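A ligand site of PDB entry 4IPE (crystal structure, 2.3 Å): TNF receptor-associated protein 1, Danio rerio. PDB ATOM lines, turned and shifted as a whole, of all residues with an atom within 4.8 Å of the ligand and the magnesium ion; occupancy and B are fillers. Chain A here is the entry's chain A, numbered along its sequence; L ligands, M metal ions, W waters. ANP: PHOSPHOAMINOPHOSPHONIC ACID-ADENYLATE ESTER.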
ATOM      1  N   GLU A 130      26.091  -8.839  21.417  1.00  0.00           N
ATOM      2  CA  GLU A 130      26.271 -10.204  20.958  1.00  0.00           C
ATOM      3  C   GLU A 130      27.578 -10.861  21.452  1.00  0.00           C
ATOM      4  O   GLU A 130      27.548 -11.993  21.957  1.00  0.00           O
ATOM      5  CB  GLU A 130      26.150 -10.291  19.419  1.00  0.00           C
ATOM      6  CG  GLU A 130      24.702 -10.064  18.888  1.00  0.00           C
ATOM      7  CD  GLU A 130      23.639 -10.820  19.723  1.00  0.00           C
ATOM      8  OE1 GLU A 130      23.636 -12.076  19.698  1.00  0.00           O
ATOM      9  OE2 GLU A 130      22.802 -10.145  20.375  1.00  0.00           O
ATOM     10  N   ASN A 134      28.111 -13.954  24.065  1.00  0.00           N
ATOM     11  CA  ASN A 134      28.930 -15.130  23.790  1.00  0.00           C
ATOM     12  C   ASN A 134      29.963 -15.408  24.894  1.00  0.00           C
ATOM     13  O   ASN A 134      30.215 -16.572  25.263  1.00  0.00           O
ATOM     14  CB  ASN A 134      29.583 -15.014  22.427  1.00  0.00           C
ATOM     15  CG  ASN A 134      28.576 -15.181  21.311  1.00  0.00           C
ATOM     16  OD1 ASN A 134      27.513 -15.787  21.532  1.00  0.00           O
ATOM     17  ND2 ASN A 134      28.874 -14.640  20.097  1.00  0.00           N
ATOM     18  N   GLY A 135      30.551 -14.347  25.424  1.00  0.00           N
ATOM     19  CA  GLY A 135      31.561 -14.488  26.458  1.00  0.00           C
ATOM     20  C   GLY A 135      30.881 -15.019  27.700  1.00  0.00           C
ATOM     21  O   GLY A 135      31.420 -15.914  28.363  1.00  0.00           O
ATOM     22  N   ASP A 137      28.135 -16.829  27.775  1.00  0.00           N
ATOM     23  CA  ASP A 137      27.806 -18.233  27.524  1.00  0.00           C
ATOM     24  C   ASP A 137      29.021 -19.148  27.735  1.00  0.00           C
ATOM     25  O   ASP A 137      28.903 -20.226  28.324  1.00  0.00           O
ATOM     26  CB  ASP A 137      27.245 -18.404  26.121  1.00  0.00           C
ATOM     27  CG  ASP A 137      25.864 -17.757  25.949  1.00  0.00           C
ATOM     28  OD1 ASP A 137      25.240 -17.383  26.969  1.00  0.00           O
ATOM     29  OD2 ASP A 137      25.422 -17.620  24.787  1.00  0.00           O
ATOM     30  N   ALA A 138      30.179 -18.718  27.235  1.00  0.00           N
ATOM     31  CA  ALA A 138      31.419 -19.478  27.349  1.00  0.00           C
ATOM     32  C   ALA A 138      31.793 -19.661  28.830  1.00  0.00           C
ATOM     33  O   ALA A 138      32.212 -20.736  29.250  1.00  0.00           O
ATOM     34  CB  ALA A 138      32.561 -18.738  26.589  1.00  0.00           C
ATOM     35  N   LYS A 141      29.327 -22.077  30.444  1.00  0.00           N
ATOM     36  CA  LYS A 141      29.627 -23.482  30.187  1.00  0.00           C
ATOM     37  C   LYS A 141      30.818 -23.994  31.014  1.00  0.00           C
ATOM     38  O   LYS A 141      30.868 -25.155  31.403  1.00  0.00           O
ATOM     39  CB  LYS A 141      29.935 -23.686  28.716  1.00  0.00           C
ATOM     40  CG  LYS A 141      28.762 -23.461  27.791  1.00  0.00           C
ATOM     41  CD  LYS A 141      29.285 -23.466  26.352  1.00  0.00           C
ATOM     42  CE  LYS A 141      28.254 -23.004  25.361  1.00  0.00           C
ATOM     43  NZ  LYS A 141      28.806 -23.125  23.989  1.00  0.00           N
ATOM     44  N   ASP A 173      37.281 -13.362  26.900  1.00  0.00           N
ATOM     45  CA  ASP A 173      36.641 -14.011  28.041  1.00  0.00           C
ATOM     46  C   ASP A 173      37.527 -15.163  28.505  1.00  0.00           C
ATOM     47  O   ASP A 173      38.283 -15.714  27.687  1.00  0.00           O
ATOM     48  CB  ASP A 173      35.251 -14.548  27.665  1.00  0.00           C
ATOM     49  CG  ASP A 173      35.317 -15.681  26.649  1.00  0.00           C
ATOM     50  OD1 ASP A 173      35.769 -16.791  27.015  1.00  0.00           O
ATOM     51  OD2 ASP A 173      34.909 -15.476  25.475  1.00  0.00           O
ATOM     52  N   VAL A 176      35.186 -21.237  28.323  1.00  0.00           N
ATOM     53  CA  VAL A 176      35.519 -22.592  27.931  1.00  0.00           C
ATOM     54  C   VAL A 176      36.405 -22.701  26.671  1.00  0.00           C
ATOM     55  O   VAL A 176      37.063 -23.720  26.486  1.00  0.00           O
ATOM     56  CB  VAL A 176      34.212 -23.394  27.785  1.00  0.00           C
ATOM     57  CG1 VAL A 176      33.565 -23.108  26.445  1.00  0.00           C
ATOM     58  CG2 VAL A 176      34.445 -24.841  27.986  1.00  0.00           C
ATOM     59  N   GLY A 177      36.430 -21.663  25.839  1.00  0.00           N
ATOM     60  CA  GLY A 177      37.316 -21.672  24.673  1.00  0.00           C
ATOM     61  C   GLY A 177      36.856 -22.641  23.597  1.00  0.00           C
ATOM     62  O   GLY A 177      35.792 -23.231  23.721  1.00  0.00           O
ATOM     63  N   MET A 178      37.657 -22.790  22.528  1.00  0.00           N
ATOM     64  CA  MET A 178      37.259 -23.543  21.337  1.00  0.00           C
ATOM     65  C   MET A 178      38.487 -24.221  20.733  1.00  0.00           C
ATOM     66  O   MET A 178      39.511 -23.560  20.510  1.00  0.00           O
ATOM     67  CB  MET A 178      36.621 -22.616  20.269  1.00  0.00           C
ATOM     68  CG  MET A 178      35.112 -22.308  20.410  1.00  0.00           C
ATOM     69  SD  MET A 178      34.477 -21.143  19.141  1.00  0.00           S
ATOM     70  CE  MET A 178      35.293 -19.588  19.588  1.00  0.00           C
ATOM     71  N   ASN A 186      31.514 -24.094  14.724  1.00  0.00           N
ATOM     72  CA  ASN A 186      30.659 -23.076  15.316  1.00  0.00           C
ATOM     73  C   ASN A 186      30.766 -21.706  14.663  1.00  0.00           C
ATOM     74  O   ASN A 186      29.744 -21.052  14.464  1.00  0.00           O
ATOM     75  CB  ASN A 186      30.914 -22.974  16.812  1.00  0.00           C
ATOM     76  CG  ASN A 186      30.459 -24.200  17.551  1.00  0.00           C
ATOM     77  OD1 ASN A 186      29.388 -24.743  17.285  1.00  0.00           O
ATOM     78  ND2 ASN A 186      31.294 -24.660  18.469  1.00  0.00           N
ATOM     79  N   LEU A 187      31.983 -21.289  14.320  1.00  0.00           N
ATOM     80  CA  LEU A 187      32.160 -19.979  13.692  1.00  0.00           C
ATOM     81  C   LEU A 187      31.933 -20.055  12.181  1.00  0.00           C
ATOM     82  O   LEU A 187      31.346 -19.147  11.605  1.00  0.00           O
ATOM     83  CB  LEU A 187      33.552 -19.400  13.973  1.00  0.00           C
ATOM     84  CG  LEU A 187      33.870 -19.001  15.425  1.00  0.00           C
ATOM     85  CD1 LEU A 187      35.181 -18.202  15.514  1.00  0.00           C
ATOM     86  CD2 LEU A 187      32.699 -18.264  16.087  1.00  0.00           C
ATOM     87  N   ARG A 192      24.481 -22.531  13.081  1.00  0.00           N
ATOM     88  CA  ARG A 192      24.877 -23.626  13.957  1.00  0.00           C
ATOM     89  C   ARG A 192      25.297 -23.015  15.271  1.00  0.00           C
ATOM     90  O   ARG A 192      26.106 -22.090  15.308  1.00  0.00           O
ATOM     91  CB  ARG A 192      25.979 -24.505  13.386  1.00  0.00           C
ATOM     92  CG  ARG A 192      26.359 -25.593  14.373  1.00  0.00           C
ATOM     93  CD  ARG A 192      27.301 -26.602  13.800  1.00  0.00           C
ATOM     94  NE  ARG A 192      26.729 -27.233  12.621  1.00  0.00           N
ATOM     95  CZ  ARG A 192      27.454 -27.841  11.677  1.00  0.00           C
ATOM     96  NH1 ARG A 192      28.772 -27.890  11.797  1.00  0.00           N
ATOM     97  NH2 ARG A 192      26.863 -28.388  10.631  1.00  0.00           N
ATOM     98  N   SER A 193      24.708 -23.522  16.343  1.00  0.00           N
ATOM     99  CA  SER A 193      24.891 -22.990  17.686  1.00  0.00           C
ATOM    100  C   SER A 193      25.393 -24.089  18.622  1.00  0.00           C
ATOM    101  O   SER A 193      24.638 -24.953  18.991  1.00  0.00           O
ATOM    102  CB  SER A 193      23.563 -22.465  18.219  1.00  0.00           C
ATOM    103  OG  SER A 193      23.674 -21.980  19.545  1.00  0.00           O
ATOM    104  N   GLY A 194      26.675 -24.046  18.986  1.00  0.00           N
ATOM    105  CA  GLY A 194      27.180 -24.923  20.009  1.00  0.00           C
ATOM    106  C   GLY A 194      26.441 -24.717  21.332  1.00  0.00           C
ATOM    107  O   GLY A 194      26.210 -25.671  22.074  1.00  0.00           O
ATOM    108  N   SER A 195      26.067 -23.471  21.633  1.00  0.00           N
ATOM    109  CA  SER A 195      25.407 -23.193  22.917  1.00  0.00           C
ATOM    110  C   SER A 195      24.008 -23.800  22.981  1.00  0.00           C
ATOM    111  O   SER A 195      23.591 -24.291  24.028  1.00  0.00           O
ATOM    112  CB  SER A 195      25.351 -21.678  23.193  1.00  0.00           C
ATOM    113  OG  SER A 195      26.653 -21.142  23.365  1.00  0.00           O
ATOM    114  N   ILE A 213      22.429 -17.577  26.964  1.00  0.00           N
ATOM    115  CA  ILE A 213      21.707 -16.577  26.184  1.00  0.00           C
ATOM    116  C   ILE A 213      21.472 -17.006  24.714  1.00  0.00           C
ATOM    117  O   ILE A 213      20.364 -16.893  24.186  1.00  0.00           O
ATOM    118  CB  ILE A 213      22.494 -15.214  26.226  1.00  0.00           C
ATOM    119  CG1 ILE A 213      22.655 -14.718  27.677  1.00  0.00           C
ATOM    120  CG2 ILE A 213      21.832 -14.174  25.289  1.00  0.00           C
ATOM    121  CD1 ILE A 213      23.923 -13.894  27.970  1.00  0.00           C
ATOM    122  N   GLY A 214      22.513 -17.505  24.051  1.00  0.00           N
ATOM    123  CA  GLY A 214      22.428 -17.821  22.628  1.00  0.00           C
ATOM    124  C   GLY A 214      21.505 -18.930  22.151  1.00  0.00           C
ATOM    125  O   GLY A 214      21.417 -19.993  22.772  1.00  0.00           O
ATOM    126  N   GLN A 215      20.847 -18.681  21.006  1.00  0.00           N
ATOM    127  CA  GLN A 215      19.847 -19.594  20.427  1.00  0.00           C
ATOM    128  C   GLN A 215      19.991 -19.824  18.917  1.00  0.00           C
ATOM    129  O   GLN A 215      19.772 -20.930  18.437  1.00  0.00           O
ATOM    130  CB  GLN A 215      18.466 -18.953  20.597  1.00  0.00           C
ATOM    131  CG  GLN A 215      17.931 -18.857  21.990  1.00  0.00           C
ATOM    132  CD  GLN A 215      16.488 -18.360  22.003  1.00  0.00           C
ATOM    133  OE1 GLN A 215      15.789 -18.454  20.997  1.00  0.00           O
ATOM    134  NE2 GLN A 215      16.042 -17.840  23.142  1.00  0.00           N
ATOM    135  N   PHE A 216      20.310 -18.767  18.185  1.00  0.00           N
ATOM    136  CA  PHE A 216      20.128 -18.811  16.741  1.00  0.00           C
ATOM    137  C   PHE A 216      21.339 -19.243  15.948  1.00  0.00           C
ATOM    138  O   PHE A 216      21.178 -19.746  14.839  1.00  0.00           O
ATOM    139  CB  PHE A 216      19.657 -17.438  16.245  1.00  0.00           C
ATOM    140  CG  PHE A 216      18.393 -16.975  16.913  1.00  0.00           C
ATOM    141  CD1 PHE A 216      17.197 -17.627  16.687  1.00  0.00           C
ATOM    142  CD2 PHE A 216      18.400 -15.865  17.755  1.00  0.00           C
ATOM    143  CE1 PHE A 216      16.027 -17.200  17.301  1.00  0.00           C
ATOM    144  CE2 PHE A 216      17.238 -15.440  18.375  1.00  0.00           C
ATOM    145  CZ  PHE A 216      16.046 -16.121  18.153  1.00  0.00           C
ATOM    146  N   GLY A 217      22.537 -19.039  16.485  1.00  0.00           N
ATOM    147  CA  GLY A 217      23.739 -19.322  15.727  1.00  0.00           C
ATOM    148  C   GLY A 217      24.076 -18.236  14.702  1.00  0.00           C
ATOM    149  O   GLY A 217      24.622 -18.548  13.651  1.00  0.00           O
ATOM    150  N   VAL A 218      23.765 -16.976  14.988  1.00  0.00           N
ATOM    151  CA  VAL A 218      24.106 -15.913  14.054  1.00  0.00           C
ATOM    152  C   VAL A 218      24.729 -14.694  14.713  1.00  0.00           C
ATOM    153  O   VAL A 218      25.254 -13.825  14.028  1.00  0.00           O
ATOM    154  CB  VAL A 218      22.865 -15.374  13.250  1.00  0.00           C
ATOM    155  CG1 VAL A 218      22.115 -16.500  12.532  1.00  0.00           C
ATOM    156  CG2 VAL A 218      21.970 -14.519  14.147  1.00  0.00           C
ATOM    157  N   GLY A 219      24.667 -14.602  16.040  1.00  0.00           N
ATOM    158  CA  GLY A 219      25.062 -13.369  16.691  1.00  0.00           C
ATOM    159  C   GLY A 219      26.518 -12.969  16.461  1.00  0.00           C
ATOM    160  O   GLY A 219      26.846 -11.787  16.451  1.00  0.00           O
ATOM    161  N   PHE A 220      27.390 -13.952  16.283  1.00  0.00           N
ATOM    162  CA  PHE A 220      28.801 -13.683  16.048  1.00  0.00           C
ATOM    163  C   PHE A 220      29.033 -12.862  14.756  1.00  0.00           C
ATOM    164  O   PHE A 220      29.927 -12.020  14.707  1.00  0.00           O
ATOM    165  CB  PHE A 220      29.602 -14.991  16.022  1.00  0.00           C
ATOM    166  CG  PHE A 220      31.025 -14.834  15.570  1.00  0.00           C
ATOM    167  CD1 PHE A 220      31.992 -14.356  16.443  1.00  0.00           C
ATOM    168  CD2 PHE A 220      31.413 -15.177  14.281  1.00  0.00           C
ATOM    169  CE1 PHE A 220      33.304 -14.196  16.041  1.00  0.00           C
ATOM    170  CE2 PHE A 220      32.741 -15.019  13.873  1.00  0.00           C
ATOM    171  CZ  PHE A 220      33.676 -14.538  14.758  1.00  0.00           C
ATOM    172  N   TYR A 221      28.193 -13.094  13.737  1.00  0.00           N
ATOM    173  CA  TYR A 221      28.371 -12.438  12.443  1.00  0.00           C
ATOM    174  C   TYR A 221      28.074 -10.951  12.562  1.00  0.00           C
ATOM    175  O   TYR A 221      28.450 -10.162  11.699  1.00  0.00           O
ATOM    176  CB  TYR A 221      27.558 -13.146  11.351  1.00  0.00           C
ATOM    177  CG  TYR A 221      27.903 -14.633  11.338  1.00  0.00           C
ATOM    178  CD1 TYR A 221      29.172 -15.071  10.962  1.00  0.00           C
ATOM    179  CD2 TYR A 221      26.987 -15.595  11.748  1.00  0.00           C
ATOM    180  CE1 TYR A 221      29.510 -16.416  10.977  1.00  0.00           C
ATOM    181  CE2 TYR A 221      27.326 -16.963  11.772  1.00  0.00           C
ATOM    182  CZ  TYR A 221      28.588 -17.363  11.382  1.00  0.00           C
ATOM    183  OH  TYR A 221      28.913 -18.714  11.396  1.00  0.00           O
ATOM    184  N   THR A 266      38.855 -17.163  24.953  1.00  0.00           N
ATOM    185  CA  THR A 266      38.719 -16.684  23.598  1.00  0.00           C
ATOM    186  C   THR A 266      38.909 -15.164  23.520  1.00  0.00           C
ATOM    187  O   THR A 266      38.333 -14.397  24.300  1.00  0.00           O
ATOM    188  CB  THR A 266      37.316 -17.041  23.062  1.00  0.00           C
ATOM    189  OG1 THR A 266      37.120 -18.466  23.205  1.00  0.00           O
ATOM    190  CG2 THR A 266      37.153 -16.673  21.611  1.00  0.00           C
ATOM    191  N   ILE A 268      38.867 -11.877  20.833  1.00  0.00           N
ATOM    192  CA  ILE A 268      38.343 -11.490  19.539  1.00  0.00           C
ATOM    193  C   ILE A 268      38.743 -10.057  19.238  1.00  0.00           C
ATOM    194  O   ILE A 268      38.441  -9.139  20.024  1.00  0.00           O
ATOM    195  CB  ILE A 268      36.811 -11.635  19.492  1.00  0.00           C
ATOM    196  CG1 ILE A 268      36.418 -13.075  19.868  1.00  0.00           C
ATOM    197  CG2 ILE A 268      36.277 -11.233  18.130  1.00  0.00           C
ATOM    198  CD1 ILE A 268      34.917 -13.353  19.829  1.00  0.00           C
ATOM    199  N   ARG A 417      16.609  -9.892  18.238  1.00  0.00           N
ATOM    200  CA  ARG A 417      16.688  -9.728  19.683  1.00  0.00           C
ATOM    201  C   ARG A 417      16.314  -8.326  20.176  1.00  0.00           C
ATOM    202  O   ARG A 417      16.750  -7.869  21.240  1.00  0.00           O
ATOM    203  CB  ARG A 417      18.077 -10.090  20.208  1.00  0.00           C
ATOM    204  CG  ARG A 417      18.395 -11.548  20.051  1.00  0.00           C
ATOM    205  CD  ARG A 417      19.833 -11.862  20.436  1.00  0.00           C
ATOM    206  NE  ARG A 417      20.011 -13.301  20.440  1.00  0.00           N
ATOM    207  CZ  ARG A 417      19.629 -14.071  21.437  1.00  0.00           C
ATOM    208  NH1 ARG A 417      19.068 -13.548  22.546  1.00  0.00           N
ATOM    209  NH2 ARG A 417      19.812 -15.383  21.365  1.00  0.00           N
HETATM  210  PG  ANP L   1      22.793 -16.567  18.999  1.00  0.00           P
HETATM  211  O1G ANP L   1      22.808 -16.200  17.546  1.00  0.00           O
HETATM  212  O2G ANP L   1      23.699 -15.546  19.787  1.00  0.00           O
HETATM  213  O3G ANP L   1      21.322 -16.479  19.580  1.00  0.00           O
HETATM  214  PB  ANP L   1      24.922 -18.509  19.325  1.00  0.00           P
HETATM  215  O1B ANP L   1      25.156 -19.988  19.466  1.00  0.00           O
HETATM  216  O2B ANP L   1      25.615 -17.764  20.504  1.00  0.00           O
HETATM  217  N3B ANP L   1      23.273 -18.175  19.285  1.00  0.00           N
HETATM  218  PA  ANP L   1      26.867 -17.242  17.789  1.00  0.00           P
HETATM  219  O1A ANP L   1      26.787 -15.999  18.628  1.00  0.00           O
HETATM  220  O2A ANP L   1      26.955 -16.973  16.294  1.00  0.00           O
HETATM  221  O3A ANP L   1      25.592 -18.159  17.946  1.00  0.00           O
HETATM  222  O5' ANP L   1      28.082 -18.136  18.262  1.00  0.00           O
HETATM  223  C5' ANP L   1      28.281 -19.366  17.519  1.00  0.00           C
HETATM  224  C4' ANP L   1      28.880 -20.418  18.437  1.00  0.00           C
HETATM  225  O4' ANP L   1      30.313 -20.208  18.533  1.00  0.00           O
HETATM  226  C3' ANP L   1      28.373 -20.450  19.862  1.00  0.00           C
HETATM  227  O3' ANP L   1      27.172 -21.211  20.010  1.00  0.00           O
HETATM  228  C2' ANP L   1      29.553 -21.089  20.604  1.00  0.00           C
HETATM  229  O2' ANP L   1      29.529 -22.490  20.364  1.00  0.00           O
HETATM  230  C1' ANP L   1      30.753 -20.507  19.845  1.00  0.00           C
HETATM  231  N9  ANP L   1      31.293 -19.302  20.443  1.00  0.00           N
HETATM  232  C8  ANP L   1      31.035 -17.995  20.085  1.00  0.00           C
HETATM  233  N7  ANP L   1      31.676 -17.107  20.823  1.00  0.00           N
HETATM  234  C5  ANP L   1      32.413 -17.882  21.708  1.00  0.00           C
HETATM  235  C6  ANP L   1      33.308 -17.543  22.731  1.00  0.00           C
HETATM  236  N6  ANP L   1      33.622 -16.280  23.069  1.00  0.00           N
HETATM  237  N1  ANP L   1      33.876 -18.552  23.426  1.00  0.00           N
HETATM  238  C2  ANP L   1      33.562 -19.815  23.105  1.00  0.00           C
HETATM  239  N3  ANP L   1      32.749 -20.249  22.151  1.00  0.00           N
HETATM  240  C4  ANP L   1      32.187 -19.222  21.486  1.00  0.00           C
HETATM  241 MG    MG M   1      25.666 -15.660  20.493  1.00  0.00          MG
HETATM  242  O   HOH W   1      26.862 -18.608  22.749  1.00  0.00           O
HETATM  243  O   HOH W   2      31.870 -14.353  20.079  1.00  0.00           O
HETATM  244  O   HOH W   3      25.932 -13.588  20.281  1.00  0.00           O
HETATM  245  O   HOH W   4      35.863 -18.718  25.345  1.00  0.00           O
HETATM  246  O   HOH W   5      22.681 -14.064  22.128  1.00  0.00           O
HETATM  247  O   HOH W   6      31.755 -22.993  22.006  1.00  0.00           O
HETATM  248  O   HOH W   7      29.705 -18.639  23.357  1.00  0.00           O
HETATM  249  O   HOH W   8      21.818 -13.585  18.234  1.00  0.00           O
HETATM  250  O   HOH W   9      32.769 -13.481  22.605  1.00  0.00           O
HETATM  251  O   HOH W  10      30.747 -20.990  24.243  1.00  0.00           O
HETATM  252  O   HOH W  11      25.019 -15.710  22.533  1.00  0.00           O
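Water W3 bridges OE1 of Glu 130 (2.8 Å) and ND2 of Asn 134 (3.1 Å).
Water W11 bridges OD2 of Asp 137 (3.0 Å) and N of Gly 214 (3.4 Å).
Water W1 lies within hydrogen-bond range of OG of Ser 195 (2.6 Å) and OD2 of Asp 137 (2.7 Å).
Water W4 lies within hydrogen-bond range of the side-chain hydroxyl of Thr 266 (2.5 Å), the side-chain carboxylate of Asp 173 (2.6 Å), a nitrogen (N1) of the ligand (2.8 Å) and the backbone NH of Gly 177 (3.0 Å).
Water W8 lies within hydrogen-bond range of the side-chain carboxylate of Glu 130 (2.8 Å), the guanidinium group of Arg 417 (2.9 Å) and an oxygen (O1G) of the ligand (2.9 Å).
Water W5 lies within hydrogen-bond range of the guanidinium group (NH2) of Arg 417 and the side-chain carboxylate (OE1) of Glu 130.
OE1 of Glu 130 lies close to O2G of the ligand (3.5 Å).
The side-chain sulfur of Met 178 lies close to a nitrogen (N3) of the ligand.
Ala 138 touches the ligand.
Lys 141 touches the ligand (NZ to O2', 3.8 Å).
Leu 187 touches the ligand (CD2 to O4', 3.9 Å).
Gly 214 touches the ligand (C to N3B, 3.5 Å).
Hydrophobic or aromatic side chains that line the ligand: Ala 138, Met 178, Leu 187, Phe 216, Val 218 and Phe 220.
20 residues have an atom within 4 Å of the ligand: Glu 130, Asn 134, Ala 138, Lys 141, Asp 173, Met 178, Asn 186, Leu 187, Ser 193, Gly 194, Ser 195, Gly 214, Gln 215, Phe 216, Gly 217, Val 218, Gly 219, Phe 220, Thr 266 and Arg 417.
The nearest printed residue that does not touch the ligand is Gly 177 (4.1 Å).
Of the 28 residues printed, 1 comes within 4 Å of the magnesium ion.
An oxygen (O3') of the ligand sits at hydrogen-bond distance from the backbone NH (N) of Ser 195 (3.0 Å).
The backbone NH of Gly 217 sits at hydrogen-bond distance from an oxygen (O1G) of the ligand (3.0 Å).
An oxygen (O3') of the ligand is in hydrogen-bond range of the backbone NH of Gly 194, at 3.1 Å.
An oxygen (O2A) of the ligand lies within hydrogen-bond range of the backbone NH of Phe 220 (3.1 Å).
OG of Ser 195 is in hydrogen-bond range of O3' of the ligand.
O1B of the ligand sits at hydrogen-bond distance from OG of Ser 193, at 2.5 Å.
An oxygen (O2') of the ligand is in hydrogen-bond range of the side-chain amide nitrogen (ND2) of Asn 186, at 3.4 Å.
O3G of the ligand is in salt-bridge range of NH2 of Arg 417 (2.6 Å).
The backbone NH (N) of Gln 215 lies within hydrogen-bond range of an oxygen (O3G) of the ligand.
N of Phe 216 sits at hydrogen-bond distance from O3G of the ligand, 2.9 Å away.
The side-chain carboxylate (OD2) of Asp 173 lies within hydrogen-bond range of a nitrogen (N6) of the ligand, at 2.8 Å.
The backbone NH of Gly 219 lies within hydrogen-bond range of an oxygen (O1G) of the ligand, at 2.9 Å.
The backbone NH of Val 218 sits at hydrogen-bond distance from an oxygen (O1G) of the ligand, at 2.8 Å.
The side-chain hydroxyl of Thr 266 lies within hydrogen-bond range of a nitrogen (N1) of the ligand (3.3 Å).
The magnesium ion is bound by an oxygen (O2G) of the ligand (2.1 Å), water W3 (2.1 Å), an oxygen (O2B) of the ligand (2.1 Å), the side-chain amide oxygen (OD1) of Asn 134 (2.1 Å), water W11 (2.1 Å) and an oxygen (O1A) of the ligand (2.2 Å).
The guanidinium group of Arg 417 is in salt-bridge range of the side-chain carboxylate of Glu 130, 3.9 Å away.
The guanidinium group (NH2) of Arg 417 is in hydrogen-bond range of the backbone carbonyl oxygen (O) of Ile 213.
The backbone carbonyl oxygen of Leu 187 is in hydrogen-bond range of the side-chain hydroxyl of Tyr 221, 2.5 Å away.
The side-chain carboxylate (OD2) of Asp 137 is in hydrogen-bond range of the backbone NH (N) of Gly 214 (3.0 Å).
OD1 of Asn 186 is in hydrogen-bond range of N of Gly 194, at 3.3 Å.
The backbone carbonyl oxygen (O) of Glu 130 sits close to the side-chain amide nitrogen (ND2) of Asn 134.
The backbone carbonyl oxygen of Thr 266 is in hydrogen-bond range of the backbone NH of Asp 173 (3.0 Å).
O of Ala 138 sits at hydrogen-bond distance from N of Val 176, 3.2 Å away.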
